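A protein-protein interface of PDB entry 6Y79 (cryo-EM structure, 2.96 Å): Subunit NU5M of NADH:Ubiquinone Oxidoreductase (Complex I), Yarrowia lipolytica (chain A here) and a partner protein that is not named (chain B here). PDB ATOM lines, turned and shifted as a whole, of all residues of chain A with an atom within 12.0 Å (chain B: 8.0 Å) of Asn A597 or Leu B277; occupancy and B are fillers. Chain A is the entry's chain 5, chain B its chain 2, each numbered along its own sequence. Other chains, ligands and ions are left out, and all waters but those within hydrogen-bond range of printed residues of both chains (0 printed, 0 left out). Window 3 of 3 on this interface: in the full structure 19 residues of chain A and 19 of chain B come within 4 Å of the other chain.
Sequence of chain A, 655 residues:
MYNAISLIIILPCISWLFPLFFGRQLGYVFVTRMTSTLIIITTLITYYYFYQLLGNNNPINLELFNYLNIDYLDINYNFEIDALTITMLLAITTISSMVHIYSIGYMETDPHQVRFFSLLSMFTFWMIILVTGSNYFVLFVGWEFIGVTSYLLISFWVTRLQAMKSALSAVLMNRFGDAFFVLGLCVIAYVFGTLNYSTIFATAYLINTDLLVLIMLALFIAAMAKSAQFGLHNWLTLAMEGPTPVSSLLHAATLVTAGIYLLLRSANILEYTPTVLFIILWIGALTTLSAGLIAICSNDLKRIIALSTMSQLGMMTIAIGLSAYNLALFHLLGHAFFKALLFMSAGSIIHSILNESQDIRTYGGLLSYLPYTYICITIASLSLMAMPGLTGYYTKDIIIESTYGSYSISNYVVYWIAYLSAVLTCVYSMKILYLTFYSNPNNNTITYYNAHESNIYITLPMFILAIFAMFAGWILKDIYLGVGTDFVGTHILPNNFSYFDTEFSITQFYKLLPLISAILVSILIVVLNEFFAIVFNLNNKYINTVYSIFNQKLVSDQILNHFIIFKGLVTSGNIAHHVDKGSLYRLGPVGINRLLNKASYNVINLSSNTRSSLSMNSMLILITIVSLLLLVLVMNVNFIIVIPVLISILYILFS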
ATOM      1  N   ARG A 586       7.453   3.090  19.384  1.00  0.00           N
ATOM      2  CA  ARG A 586       6.805   2.524  20.552  1.00  0.00           C
ATOM      3  C   ARG A 586       5.304   2.461  20.343  1.00  0.00           C
ATOM      4  O   ARG A 586       4.643   1.542  20.836  1.00  0.00           O
ATOM      5  CB  ARG A 586       7.167   3.342  21.786  1.00  0.00           C
ATOM      6  CG  ARG A 586       6.940   2.620  23.079  1.00  0.00           C
ATOM      7  CD  ARG A 586       7.642   1.282  23.103  1.00  0.00           C
ATOM      8  NE  ARG A 586       9.085   1.423  23.007  1.00  0.00           N
ATOM      9  CZ  ARG A 586       9.881   1.580  24.057  1.00  0.00           C
ATOM     10  NH1 ARG A 586       9.366   1.619  25.274  1.00  0.00           N
ATOM     11  NH2 ARG A 586      11.186   1.696  23.892  1.00  0.00           N
ATOM     12  N   GLY A 588       4.470   2.104  17.254  1.00  0.00           N
ATOM     13  CA  GLY A 588       4.514   1.393  16.007  1.00  0.00           C
ATOM     14  C   GLY A 588       5.030  -0.011  16.194  1.00  0.00           C
ATOM     15  O   GLY A 588       4.648  -0.712  17.129  1.00  0.00           O
ATOM     16  N   PRO A 589       5.946  -0.436  15.325  1.00  0.00           N
ATOM     17  CA  PRO A 589       6.275  -1.865  15.241  1.00  0.00           C
ATOM     18  C   PRO A 589       7.128  -2.411  16.375  1.00  0.00           C
ATOM     19  O   PRO A 589       7.229  -3.636  16.496  1.00  0.00           O
ATOM     20  CB  PRO A 589       7.015  -1.969  13.906  1.00  0.00           C
ATOM     21  CG  PRO A 589       7.522  -0.620  13.641  1.00  0.00           C
ATOM     22  CD  PRO A 589       6.555   0.338  14.233  1.00  0.00           C
ATOM     23  N   VAL A 590       7.728  -1.569  17.207  1.00  0.00           N
ATOM     24  CA  VAL A 590       8.654  -2.025  18.240  1.00  0.00           C
ATOM     25  C   VAL A 590       7.906  -2.209  19.555  1.00  0.00           C
ATOM     26  O   VAL A 590       8.219  -3.108  20.343  1.00  0.00           O
ATOM     27  CB  VAL A 590       9.838  -1.046  18.360  1.00  0.00           C
ATOM     28  CG1 VAL A 590      10.829  -1.473  19.413  1.00  0.00           C
ATOM     29  CG2 VAL A 590      10.557  -1.015  17.057  1.00  0.00           C
ATOM     30  N   GLY A 591       6.872  -1.406  19.778  1.00  0.00           N
ATOM     31  CA  GLY A 591       6.083  -1.536  20.984  1.00  0.00           C
ATOM     32  C   GLY A 591       4.983  -2.564  20.857  1.00  0.00           C
ATOM     33  O   GLY A 591       4.630  -3.247  21.825  1.00  0.00           O
ATOM     34  N   ILE A 592       4.436  -2.683  19.648  1.00  0.00           N
ATOM     35  CA  ILE A 592       3.387  -3.661  19.391  1.00  0.00           C
ATOM     36  C   ILE A 592       3.942  -5.078  19.463  1.00  0.00           C
ATOM     37  O   ILE A 592       3.268  -5.978  19.968  1.00  0.00           O
ATOM     38  CB  ILE A 592       2.707  -3.335  18.046  1.00  0.00           C
ATOM     39  CG1 ILE A 592       1.890  -2.064  18.227  1.00  0.00           C
ATOM     40  CG2 ILE A 592       1.808  -4.453  17.560  1.00  0.00           C
ATOM     41  CD1 ILE A 592       1.104  -1.611  17.054  1.00  0.00           C
ATOM     42  N   ASN A 593       5.190  -5.282  19.036  1.00  0.00           N
ATOM     43  CA  ASN A 593       5.836  -6.585  19.163  1.00  0.00           C
ATOM     44  C   ASN A 593       5.965  -7.006  20.623  1.00  0.00           C
ATOM     45  O   ASN A 593       5.703  -8.163  20.967  1.00  0.00           O
ATOM     46  CB  ASN A 593       7.205  -6.543  18.486  1.00  0.00           C
ATOM     47  CG  ASN A 593       7.839  -7.910  18.339  1.00  0.00           C
ATOM     48  OD1 ASN A 593       7.229  -8.932  18.618  1.00  0.00           O
ATOM     49  ND2 ASN A 593       9.083  -7.928  17.892  1.00  0.00           N
ATOM     50  N   ARG A 594       6.290  -6.064  21.505  1.00  0.00           N
ATOM     51  CA  ARG A 594       6.446  -6.396  22.914  1.00  0.00           C
ATOM     52  C   ARG A 594       5.099  -6.632  23.585  1.00  0.00           C
ATOM     53  O   ARG A 594       4.963  -7.553  24.406  1.00  0.00           O
ATOM     54  CB  ARG A 594       7.215  -5.283  23.614  1.00  0.00           C
ATOM     55  CG  ARG A 594       8.622  -5.136  23.107  1.00  0.00           C
ATOM     56  CD  ARG A 594       9.374  -4.097  23.889  1.00  0.00           C
ATOM     57  NE  ARG A 594      10.727  -3.930  23.379  1.00  0.00           N
ATOM     58  CZ  ARG A 594      11.559  -2.985  23.789  1.00  0.00           C
ATOM     59  NH1 ARG A 594      11.173  -2.128  24.718  1.00  0.00           N
ATOM     60  NH2 ARG A 594      12.775  -2.901  23.275  1.00  0.00           N
ATOM     61  N   LEU A 595       4.094  -5.823  23.230  1.00  0.00           N
ATOM     62  CA  LEU A 595       2.744  -6.010  23.757  1.00  0.00           C
ATOM     63  C   LEU A 595       2.177  -7.364  23.356  1.00  0.00           C
ATOM     64  O   LEU A 595       1.600  -8.076  24.185  1.00  0.00           O
ATOM     65  CB  LEU A 595       1.836  -4.886  23.263  1.00  0.00           C
ATOM     66  CG  LEU A 595       0.445  -4.685  23.868  1.00  0.00           C
ATOM     67  CD1 LEU A 595       0.175  -3.214  23.932  1.00  0.00           C
ATOM     68  CD2 LEU A 595      -0.648  -5.351  23.057  1.00  0.00           C
ATOM     69  N   LEU A 596       2.348  -7.742  22.086  1.00  0.00           N
ATOM     70  CA  LEU A 596       1.811  -9.006  21.605  1.00  0.00           C
ATOM     71  C   LEU A 596       2.588 -10.191  22.146  1.00  0.00           C
ATOM     72  O   LEU A 596       1.994 -11.243  22.392  1.00  0.00           O
ATOM     73  CB  LEU A 596       1.812  -9.035  20.082  1.00  0.00           C
ATOM     74  CG  LEU A 596       0.869  -8.067  19.370  1.00  0.00           C
ATOM     75  CD1 LEU A 596       0.999  -8.213  17.868  1.00  0.00           C
ATOM     76  CD2 LEU A 596      -0.561  -8.228  19.833  1.00  0.00           C
ATOM     77  N   ASN A 597       3.904 -10.035  22.334  1.00  0.00           N
ATOM     78  CA  ASN A 597       4.719 -11.045  23.002  1.00  0.00           C
ATOM     79  C   ASN A 597       4.200 -11.332  24.405  1.00  0.00           C
ATOM     80  O   ASN A 597       3.995 -12.494  24.778  1.00  0.00           O
ATOM     81  CB  ASN A 597       6.165 -10.548  23.035  1.00  0.00           C
ATOM     82  CG  ASN A 597       7.167 -11.619  23.404  1.00  0.00           C
ATOM     83  OD1 ASN A 597       6.820 -12.755  23.694  1.00  0.00           O
ATOM     84  ND2 ASN A 597       8.437 -11.245  23.395  1.00  0.00           N
ATOM     85  N   LYS A 598       3.918 -10.277  25.174  1.00  0.00           N
ATOM     86  CA  LYS A 598       3.441 -10.473  26.541  1.00  0.00           C
ATOM     87  C   LYS A 598       2.031 -11.054  26.569  1.00  0.00           C
ATOM     88  O   LYS A 598       1.759 -11.993  27.329  1.00  0.00           O
ATOM     89  CB  LYS A 598       3.508  -9.160  27.316  1.00  0.00           C
ATOM     90  CG  LYS A 598       3.038  -9.279  28.751  1.00  0.00           C
ATOM     91  CD  LYS A 598       3.877 -10.278  29.552  1.00  0.00           C
ATOM     92  CE  LYS A 598       5.268  -9.748  29.865  1.00  0.00           C
ATOM     93  NZ  LYS A 598       6.057 -10.677  30.728  1.00  0.00           N
ATOM     94  N   ALA A 599       1.131 -10.533  25.727  1.00  0.00           N
ATOM     95  CA  ALA A 599      -0.253 -11.000  25.722  1.00  0.00           C
ATOM     96  C   ALA A 599      -0.363 -12.443  25.245  1.00  0.00           C
ATOM     97  O   ALA A 599      -1.155 -13.226  25.788  1.00  0.00           O
ATOM     98  CB  ALA A 599      -1.107 -10.083  24.854  1.00  0.00           C
ATOM     99  N   SER A 600       0.470 -12.833  24.279  1.00  0.00           N
ATOM    100  CA  SER A 600       0.468 -14.208  23.804  1.00  0.00           C
ATOM    101  C   SER A 600       1.060 -15.151  24.837  1.00  0.00           C
ATOM    102  O   SER A 600       0.554 -16.263  25.017  1.00  0.00           O
ATOM    103  CB  SER A 600       1.248 -14.307  22.501  1.00  0.00           C
ATOM    104  OG  SER A 600       1.184 -15.621  21.988  1.00  0.00           O
ATOM    105  N   TYR A 601       2.133 -14.727  25.519  1.00  0.00           N
ATOM    106  CA  TYR A 601       2.720 -15.535  26.583  1.00  0.00           C
ATOM    107  C   TYR A 601       1.718 -15.785  27.701  1.00  0.00           C
ATOM    108  O   TYR A 601       1.606 -16.907  28.209  1.00  0.00           O
ATOM    109  CB  TYR A 601       3.963 -14.825  27.113  1.00  0.00           C
ATOM    110  CG  TYR A 601       4.746 -15.551  28.180  1.00  0.00           C
ATOM    111  CD1 TYR A 601       5.546 -16.636  27.861  1.00  0.00           C
ATOM    112  CD2 TYR A 601       4.719 -15.119  29.500  1.00  0.00           C
ATOM    113  CE1 TYR A 601       6.282 -17.288  28.831  1.00  0.00           C
ATOM    114  CE2 TYR A 601       5.452 -15.763  30.478  1.00  0.00           C
ATOM    115  CZ  TYR A 601       6.232 -16.847  30.136  1.00  0.00           C
ATOM    116  OH  TYR A 601       6.964 -17.501  31.103  1.00  0.00           O
ATOM    117  N   ASN A 602       0.928 -14.765  28.036  1.00  0.00           N
ATOM    118  CA  ASN A 602      -0.047 -14.901  29.108  1.00  0.00           C
ATOM    119  C   ASN A 602      -1.201 -15.814  28.707  1.00  0.00           C
ATOM    120  O   ASN A 602      -1.605 -16.693  29.481  1.00  0.00           O
ATOM    121  CB  ASN A 602      -0.543 -13.522  29.525  1.00  0.00           C
ATOM    122  CG  ASN A 602       0.506 -12.745  30.295  1.00  0.00           C
ATOM    123  OD1 ASN A 602       0.799 -11.596  29.986  1.00  0.00           O
ATOM    124  ND2 ASN A 602       1.085 -13.380  31.302  1.00  0.00           N
ATOM    125  N   VAL A 603      -1.725 -15.661  27.489  1.00  0.00           N
ATOM    126  CA  VAL A 603      -2.830 -16.537  27.102  1.00  0.00           C
ATOM    127  C   VAL A 603      -2.387 -17.952  26.768  1.00  0.00           C
ATOM    128  O   VAL A 603      -3.227 -18.854  26.727  1.00  0.00           O
ATOM    129  CB  VAL A 603      -3.634 -15.990  25.916  1.00  0.00           C
ATOM    130  CG1 VAL A 603      -4.160 -14.649  26.255  1.00  0.00           C
ATOM    131  CG2 VAL A 603      -2.793 -15.930  24.678  1.00  0.00           C
ATOM    132  N   ILE A 604      -1.101 -18.187  26.531  1.00  0.00           N
ATOM    133  CA  ILE A 604      -0.653 -19.563  26.361  1.00  0.00           C
ATOM    134  C   ILE A 604      -0.409 -20.212  27.717  1.00  0.00           C
ATOM    135  O   ILE A 604      -0.779 -21.370  27.938  1.00  0.00           O
ATOM    136  CB  ILE A 604       0.584 -19.595  25.447  1.00  0.00           C
ATOM    137  CG1 ILE A 604       0.163 -19.328  24.012  1.00  0.00           C
ATOM    138  CG2 ILE A 604       1.284 -20.926  25.487  1.00  0.00           C
ATOM    139  CD1 ILE A 604       1.304 -18.963  23.132  1.00  0.00           C
ATOM    140  N   ASN A 605       0.146 -19.467  28.676  1.00  0.00           N
ATOM    141  CA  ASN A 605       0.287 -19.987  30.033  1.00  0.00           C
ATOM    142  C   ASN A 605      -1.011 -19.972  30.830  1.00  0.00           C
ATOM    143  O   ASN A 605      -0.974 -20.291  32.024  1.00  0.00           O
ATOM    144  CB  ASN A 605       1.341 -19.195  30.796  1.00  0.00           C
ATOM    145  CG  ASN A 605       2.718 -19.385  30.238  1.00  0.00           C
ATOM    146  OD1 ASN A 605       3.140 -20.501  29.953  1.00  0.00           O
ATOM    147  ND2 ASN A 605       3.430 -18.289  30.067  1.00  0.00           N
ATOM    148  N   LEU A 606      -2.122 -19.554  30.215  1.00  0.00           N
ATOM    149  CA  LEU A 606      -3.440 -19.673  30.834  1.00  0.00           C
ATOM    150  C   LEU A 606      -3.749 -21.105  31.287  1.00  0.00           C
ATOM    151  O   LEU A 606      -4.353 -21.307  32.346  1.00  0.00           O
ATOM    152  CB  LEU A 606      -4.498 -19.154  29.854  1.00  0.00           C
ATOM    153  CG  LEU A 606      -5.972 -18.992  30.230  1.00  0.00           C
ATOM    154  CD1 LEU A 606      -6.088 -18.144  31.479  1.00  0.00           C
ATOM    155  CD2 LEU A 606      -6.748 -18.338  29.083  1.00  0.00           C
ATOM    156  N   SER A 607      -3.326 -22.114  30.531  1.00  0.00           N
ATOM    157  CA  SER A 607      -3.551 -23.508  30.915  1.00  0.00           C
ATOM    158  C   SER A 607      -2.252 -24.294  31.066  1.00  0.00           C
ATOM    159  O   SER A 607      -2.144 -25.440  30.624  1.00  0.00           O
ATOM    160  CB  SER A 607      -4.455 -24.202  29.911  1.00  0.00           C
ATOM    161  OG  SER A 607      -3.767 -24.421  28.696  1.00  0.00           O
ATOM    162  N   SER A 608      -1.252 -23.684  31.689  1.00  0.00           N
ATOM    163  CA  SER A 608       0.041 -24.325  31.875  1.00  0.00           C
ATOM    164  C   SER A 608       0.084 -25.186  33.129  1.00  0.00           C
ATOM    165  O   SER A 608       0.892 -26.122  33.205  1.00  0.00           O
ATOM    166  CB  SER A 608       1.134 -23.259  31.951  1.00  0.00           C
ATOM    167  OG  SER A 608       0.884 -22.370  33.030  1.00  0.00           O
ATOM    168  N   LEU A 653      -6.596 -11.816  31.903  1.00  0.00           N
ATOM    169  CA  LEU A 653      -6.495 -12.842  30.871  1.00  0.00           C
ATOM    170  C   LEU A 653      -5.249 -12.638  30.024  1.00  0.00           C
ATOM    171  O   LEU A 653      -4.531 -13.595  29.718  1.00  0.00           O
ATOM    172  CB  LEU A 653      -7.753 -12.819  30.001  1.00  0.00           C
ATOM    173  CG  LEU A 653      -8.130 -13.954  29.051  1.00  0.00           C
ATOM    174  CD1 LEU A 653      -9.638 -13.992  28.952  1.00  0.00           C
ATOM    175  CD2 LEU A 653      -7.530 -13.817  27.651  1.00  0.00           C
ATOM    176  N   PHE A 654      -4.973 -11.394  29.641  1.00  0.00           N
ATOM    177  CA  PHE A 654      -3.841 -11.058  28.796  1.00  0.00           C
ATOM    178  C   PHE A 654      -2.621 -10.600  29.586  1.00  0.00           C
ATOM    179  O   PHE A 654      -1.585 -10.322  28.979  1.00  0.00           O
ATOM    180  CB  PHE A 654      -4.249  -9.979  27.790  1.00  0.00           C
ATOM    181  CG  PHE A 654      -5.278 -10.435  26.800  1.00  0.00           C
ATOM    182  CD1 PHE A 654      -4.921 -11.243  25.746  1.00  0.00           C
ATOM    183  CD2 PHE A 654      -6.597 -10.050  26.917  1.00  0.00           C
ATOM    184  CE1 PHE A 654      -5.862 -11.678  24.838  1.00  0.00           C
ATOM    185  CE2 PHE A 654      -7.539 -10.480  26.006  1.00  0.00           C
ATOM    186  CZ  PHE A 654      -7.167 -11.292  24.965  1.00  0.00           C
ATOM    187  N   SER A 655      -2.719 -10.512  30.912  1.00  0.00           N
ATOM    188  CA  SER A 655      -1.586 -10.156  31.770  1.00  0.00           C
ATOM    189  C   SER A 655      -1.738 -10.741  33.177  1.00  0.00           C
ATOM    190  O   SER A 655      -1.690 -11.949  33.373  1.00  0.00           O
ATOM    191  CB  SER A 655      -1.436  -8.634  31.872  1.00  0.00           C
ATOM    192  OG  SER A 655      -1.164  -8.068  30.635  1.00  0.00           O
ATOM    193  N   SER B 272      -6.422 -14.310  17.485  1.00  0.00           N
ATOM    194  CA  SER B 272      -5.406 -13.526  16.804  1.00  0.00           C
ATOM    195  C   SER B 272      -4.121 -13.470  17.619  1.00  0.00           C
ATOM    196  O   SER B 272      -3.044 -13.779  17.105  1.00  0.00           O
ATOM    197  CB  SER B 272      -5.941 -12.130  16.506  1.00  0.00           C
ATOM    198  OG  SER B 272      -6.199 -11.412  17.692  1.00  0.00           O
ATOM    199  N   VAL B 273      -4.207 -13.106  18.903  1.00  0.00           N
ATOM    200  CA  VAL B 273      -2.997 -13.022  19.713  1.00  0.00           C
ATOM    201  C   VAL B 273      -2.637 -14.343  20.364  1.00  0.00           C
ATOM    202  O   VAL B 273      -1.617 -14.420  21.053  1.00  0.00           O
ATOM    203  CB  VAL B 273      -3.087 -11.964  20.828  1.00  0.00           C
ATOM    204  CG1 VAL B 273      -3.465 -10.618  20.256  1.00  0.00           C
ATOM    205  CG2 VAL B 273      -4.049 -12.398  21.868  1.00  0.00           C
ATOM    206  N   GLY B 274      -3.429 -15.383  20.179  1.00  0.00           N
ATOM    207  CA  GLY B 274      -3.106 -16.645  20.802  1.00  0.00           C
ATOM    208  C   GLY B 274      -2.106 -17.455  20.016  1.00  0.00           C
ATOM    209  O   GLY B 274      -1.278 -18.157  20.598  1.00  0.00           O
ATOM    210  N   GLY B 275      -2.175 -17.376  18.695  1.00  0.00           N
ATOM    211  CA  GLY B 275      -1.323 -18.193  17.864  1.00  0.00           C
ATOM    212  C   GLY B 275      -0.098 -17.475  17.353  1.00  0.00           C
ATOM    213  O   GLY B 275       0.468 -17.861  16.331  1.00  0.00           O
ATOM    214  N   LEU B 276       0.338 -16.439  18.065  1.00  0.00           N
ATOM    215  CA  LEU B 276       1.468 -15.646  17.602  1.00  0.00           C
ATOM    216  C   LEU B 276       2.791 -16.340  17.887  1.00  0.00           C
ATOM    217  O   LEU B 276       3.564 -16.620  16.968  1.00  0.00           O
ATOM    218  CB  LEU B 276       1.433 -14.261  18.239  1.00  0.00           C
ATOM    219  CG  LEU B 276       0.394 -13.323  17.640  1.00  0.00           C
ATOM    220  CD1 LEU B 276       0.368 -12.022  18.385  1.00  0.00           C
ATOM    221  CD2 LEU B 276       0.706 -13.092  16.191  1.00  0.00           C
ATOM    222  N   LEU B 277       3.079 -16.629  19.152  1.00  0.00           N
ATOM    223  CA  LEU B 277       4.329 -17.309  19.485  1.00  0.00           C
ATOM    224  C   LEU B 277       4.082 -18.815  19.572  1.00  0.00           C
ATOM    225  O   LEU B 277       4.099 -19.440  20.626  1.00  0.00           O
ATOM    226  CB  LEU B 277       4.954 -16.718  20.747  1.00  0.00           C
ATOM    227  CG  LEU B 277       4.378 -16.474  22.137  1.00  0.00           C
ATOM    228  CD1 LEU B 277       4.758 -17.534  23.138  1.00  0.00           C
ATOM    229  CD2 LEU B 277       4.917 -15.169  22.586  1.00  0.00           C
ATOM    230  N   GLN B 278       3.859 -19.403  18.404  1.00  0.00           N
ATOM    231  CA  GLN B 278       3.633 -20.833  18.318  1.00  0.00           C
ATOM    232  C   GLN B 278       4.415 -21.436  17.171  1.00  0.00           C
ATOM    233  O   GLN B 278       4.479 -20.871  16.079  1.00  0.00           O
ATOM    234  CB  GLN B 278       2.167 -21.147  18.163  1.00  0.00           C
ATOM    235  CG  GLN B 278       1.525 -21.185  19.494  1.00  0.00           C
ATOM    236  CD  GLN B 278       0.082 -21.311  19.404  1.00  0.00           C
ATOM    237  OE1 GLN B 278      -0.443 -21.662  18.361  1.00  0.00           O
ATOM    238  NE2 GLN B 278      -0.599 -20.990  20.487  1.00  0.00           N
ATOM    239  N   ILE B 279       4.992 -22.603  17.441  1.00  0.00           N
ATOM    240  CA  ILE B 279       6.010 -23.206  16.600  1.00  0.00           C
ATOM    241  C   ILE B 279       5.569 -24.523  15.996  1.00  0.00           C
ATOM    242  O   ILE B 279       6.351 -25.151  15.287  1.00  0.00           O
ATOM    243  CB  ILE B 279       7.323 -23.400  17.382  1.00  0.00           C
ATOM    244  CG1 ILE B 279       7.159 -24.462  18.462  1.00  0.00           C
ATOM    245  CG2 ILE B 279       7.705 -22.141  18.061  1.00  0.00           C
ATOM    246  CD1 ILE B 279       8.459 -24.941  18.999  1.00  0.00           C
ATOM    247  N   LYS B 280       4.356 -24.977  16.278  1.00  0.00           N
ATOM    248  CA  LYS B 280       3.819 -26.188  15.676  1.00  0.00           C
ATOM    249  C   LYS B 280       2.783 -25.802  14.637  1.00  0.00           C
ATOM    250  O   LYS B 280       2.000 -24.877  14.849  1.00  0.00           O
ATOM    251  CB  LYS B 280       3.198 -27.101  16.723  1.00  0.00           C
ATOM    252  CG  LYS B 280       4.156 -27.549  17.791  1.00  0.00           C
ATOM    253  CD  LYS B 280       3.462 -28.461  18.761  1.00  0.00           C
ATOM    254  CE  LYS B 280       4.426 -29.045  19.753  1.00  0.00           C
ATOM    255  NZ  LYS B 280       3.734 -29.995  20.651  1.00  0.00           N
ATOM    256  N   ARG B 283      -1.042 -26.348  15.491  1.00  0.00           N
ATOM    257  CA  ARG B 283      -1.454 -25.332  16.452  1.00  0.00           C
ATOM    258  C   ARG B 283      -1.738 -24.011  15.758  1.00  0.00           C
ATOM    259  O   ARG B 283      -2.836 -23.455  15.877  1.00  0.00           O
ATOM    260  CB  ARG B 283      -0.356 -25.150  17.489  1.00  0.00           C
ATOM    261  CG  ARG B 283      -0.074 -26.372  18.281  1.00  0.00           C
ATOM    262  CD  ARG B 283      -1.186 -26.547  19.218  1.00  0.00           C
ATOM    263  NE  ARG B 283      -1.314 -25.387  20.077  1.00  0.00           N
ATOM    264  CZ  ARG B 283      -1.128 -25.428  21.383  1.00  0.00           C
ATOM    265  NH1 ARG B 283      -0.819 -26.578  21.946  1.00  0.00           N
ATOM    266  NH2 ARG B 283      -1.258 -24.335  22.118  1.00  0.00           N
ATOM    267  N   LEU B 284      -0.735 -23.494  15.048  1.00  0.00           N
ATOM    268  CA  LEU B 284      -0.766 -22.317  14.187  1.00  0.00           C
ATOM    269  C   LEU B 284      -1.971 -22.321  13.266  1.00  0.00           C
ATOM    270  O   LEU B 284      -2.624 -21.298  13.056  1.00  0.00           O
ATOM    271  CB  LEU B 284       0.509 -22.287  13.350  1.00  0.00           C
ATOM    272  CG  LEU B 284       0.857 -21.041  12.569  1.00  0.00           C
ATOM    273  CD1 LEU B 284       1.360 -20.062  13.557  1.00  0.00           C
ATOM    274  CD2 LEU B 284       1.916 -21.345  11.549  1.00  0.00           C
ATOM    275  N   TYR B 412       0.978 -14.413  11.963  1.00  0.00           N
ATOM    276  CA  TYR B 412       1.300 -15.830  11.955  1.00  0.00           C
ATOM    277  C   TYR B 412       0.846 -16.545  10.688  1.00  0.00           C
ATOM    278  O   TYR B 412       1.230 -17.696  10.487  1.00  0.00           O
ATOM    279  CB  TYR B 412       0.742 -16.508  13.213  1.00  0.00           C
ATOM    280  CG  TYR B 412      -0.759 -16.540  13.403  1.00  0.00           C
ATOM    281  CD1 TYR B 412      -1.546 -17.493  12.768  1.00  0.00           C
ATOM    282  CD2 TYR B 412      -1.375 -15.666  14.276  1.00  0.00           C
ATOM    283  CE1 TYR B 412      -2.893 -17.534  12.947  1.00  0.00           C
ATOM    284  CE2 TYR B 412      -2.732 -15.710  14.472  1.00  0.00           C
ATOM    285  CZ  TYR B 412      -3.485 -16.646  13.802  1.00  0.00           C
ATOM    286  OH  TYR B 412      -4.840 -16.694  13.984  1.00  0.00           O
ATOM    287  N   TYR B 415       4.032 -15.863   8.751  1.00  0.00           N
ATOM    288  CA  TYR B 415       5.158 -16.600   9.300  1.00  0.00           C
ATOM    289  C   TYR B 415       5.415 -17.899   8.538  1.00  0.00           C
ATOM    290  O   TYR B 415       6.573 -18.302   8.380  1.00  0.00           O
ATOM    291  CB  TYR B 415       4.892 -16.832  10.777  1.00  0.00           C
ATOM    292  CG  TYR B 415       5.829 -17.776  11.434  1.00  0.00           C
ATOM    293  CD1 TYR B 415       7.197 -17.560  11.410  1.00  0.00           C
ATOM    294  CD2 TYR B 415       5.349 -18.869  12.110  1.00  0.00           C
ATOM    295  CE1 TYR B 415       8.048 -18.431  12.014  1.00  0.00           C
ATOM    296  CE2 TYR B 415       6.187 -19.726  12.723  1.00  0.00           C
ATOM    297  CZ  TYR B 415       7.536 -19.520  12.666  1.00  0.00           C
ATOM    298  OH  TYR B 415       8.370 -20.409  13.289  1.00  0.00           O
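Val A590 touches none of the printed residues of chain B. Of chain B, only Leu B277 comes within 4 Å of Asn A597. Of the printed residues of chain B, Val A603 touches Gly B274 (3.95 Å). Of the printed residues of chain A, Val B273 touches Leu A596, Ser A600 and Phe A654. Gly B274 touches just these residues of chain A: Ser A600, Val A603 and Ile A604. No residue of chain A comes within 4 Å of Gly B275. Printed residues of chain A within 4 Å of Leu B276: Leu A596 (3.7 Å) and Ser A600 (3.996 Å). Of chain A, only Asn A597, Ser A600 and Ile A604 come within 4 Å of Leu B277. The nearest residue of chain B that does not touch Asn A597 is Leu B276 (5.7 Å). The nearest residue of chain A that does not touch Leu B277 is Tyr A601 (4.1 Å). The nearest printed residue of chain B that does not touch Val A603 is Val B273 (4.1 Å).
Printed residues of chain A that touch a printed residue of chain B: Leu A596, Asn A597, Ser A600, Val A603, Ile A604 and Phe A654. Hydrophobic or aromatic side chains of chain A that line the printed part of chain B: Leu A596, Val A603, Ile A604 and Phe A654. Hydrophobic or aromatic side chains of chain B within 4 Å of the printed part of chain A: Val B273, Leu B276 and Leu B277. Among the printed residues, 12 pairs touch across the chains. Among the printed residues, no Asp or Glu carboxylate lies within 4 Å of a Lys or Arg side-chain nitrogen of the other chain.
Among the printed residues, pairs that only touch across the chains: Leu A596 with Val B273 (3.8 Å), Leu A596 with Leu B276 (3.7 Å), Asn A597 with Leu B277 (3.3 Å), Ser A600 with Gly B274 (3.8 Å), Ser A600 with Leu B276 (3.996 Å), Ser A600 with Leu B277 (3.3 Å), Val A603 with Gly B274 (3.95 Å), Ile A604 with Gly B274 (3.7 Å), Ile A604 with Leu B277 (3.7 Å), Ile A604 with Gln B278 (3.8 Å) and Phe A654 with Val B273 (3.6 Å).
The backbone carbonyl oxygen (O) of Gly B274 lies within hydrogen-bond range of the side-chain amide nitrogen (NE2) of Gln B278 (2.9 Å). The backbone carbonyl oxygen of Phe A654 sits close to the side-chain amide oxygen of Asn A602, at 2.9 Å.
OG of Ser A600 is in hydrogen-bond range of O of Val B273 (3.2 Å).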
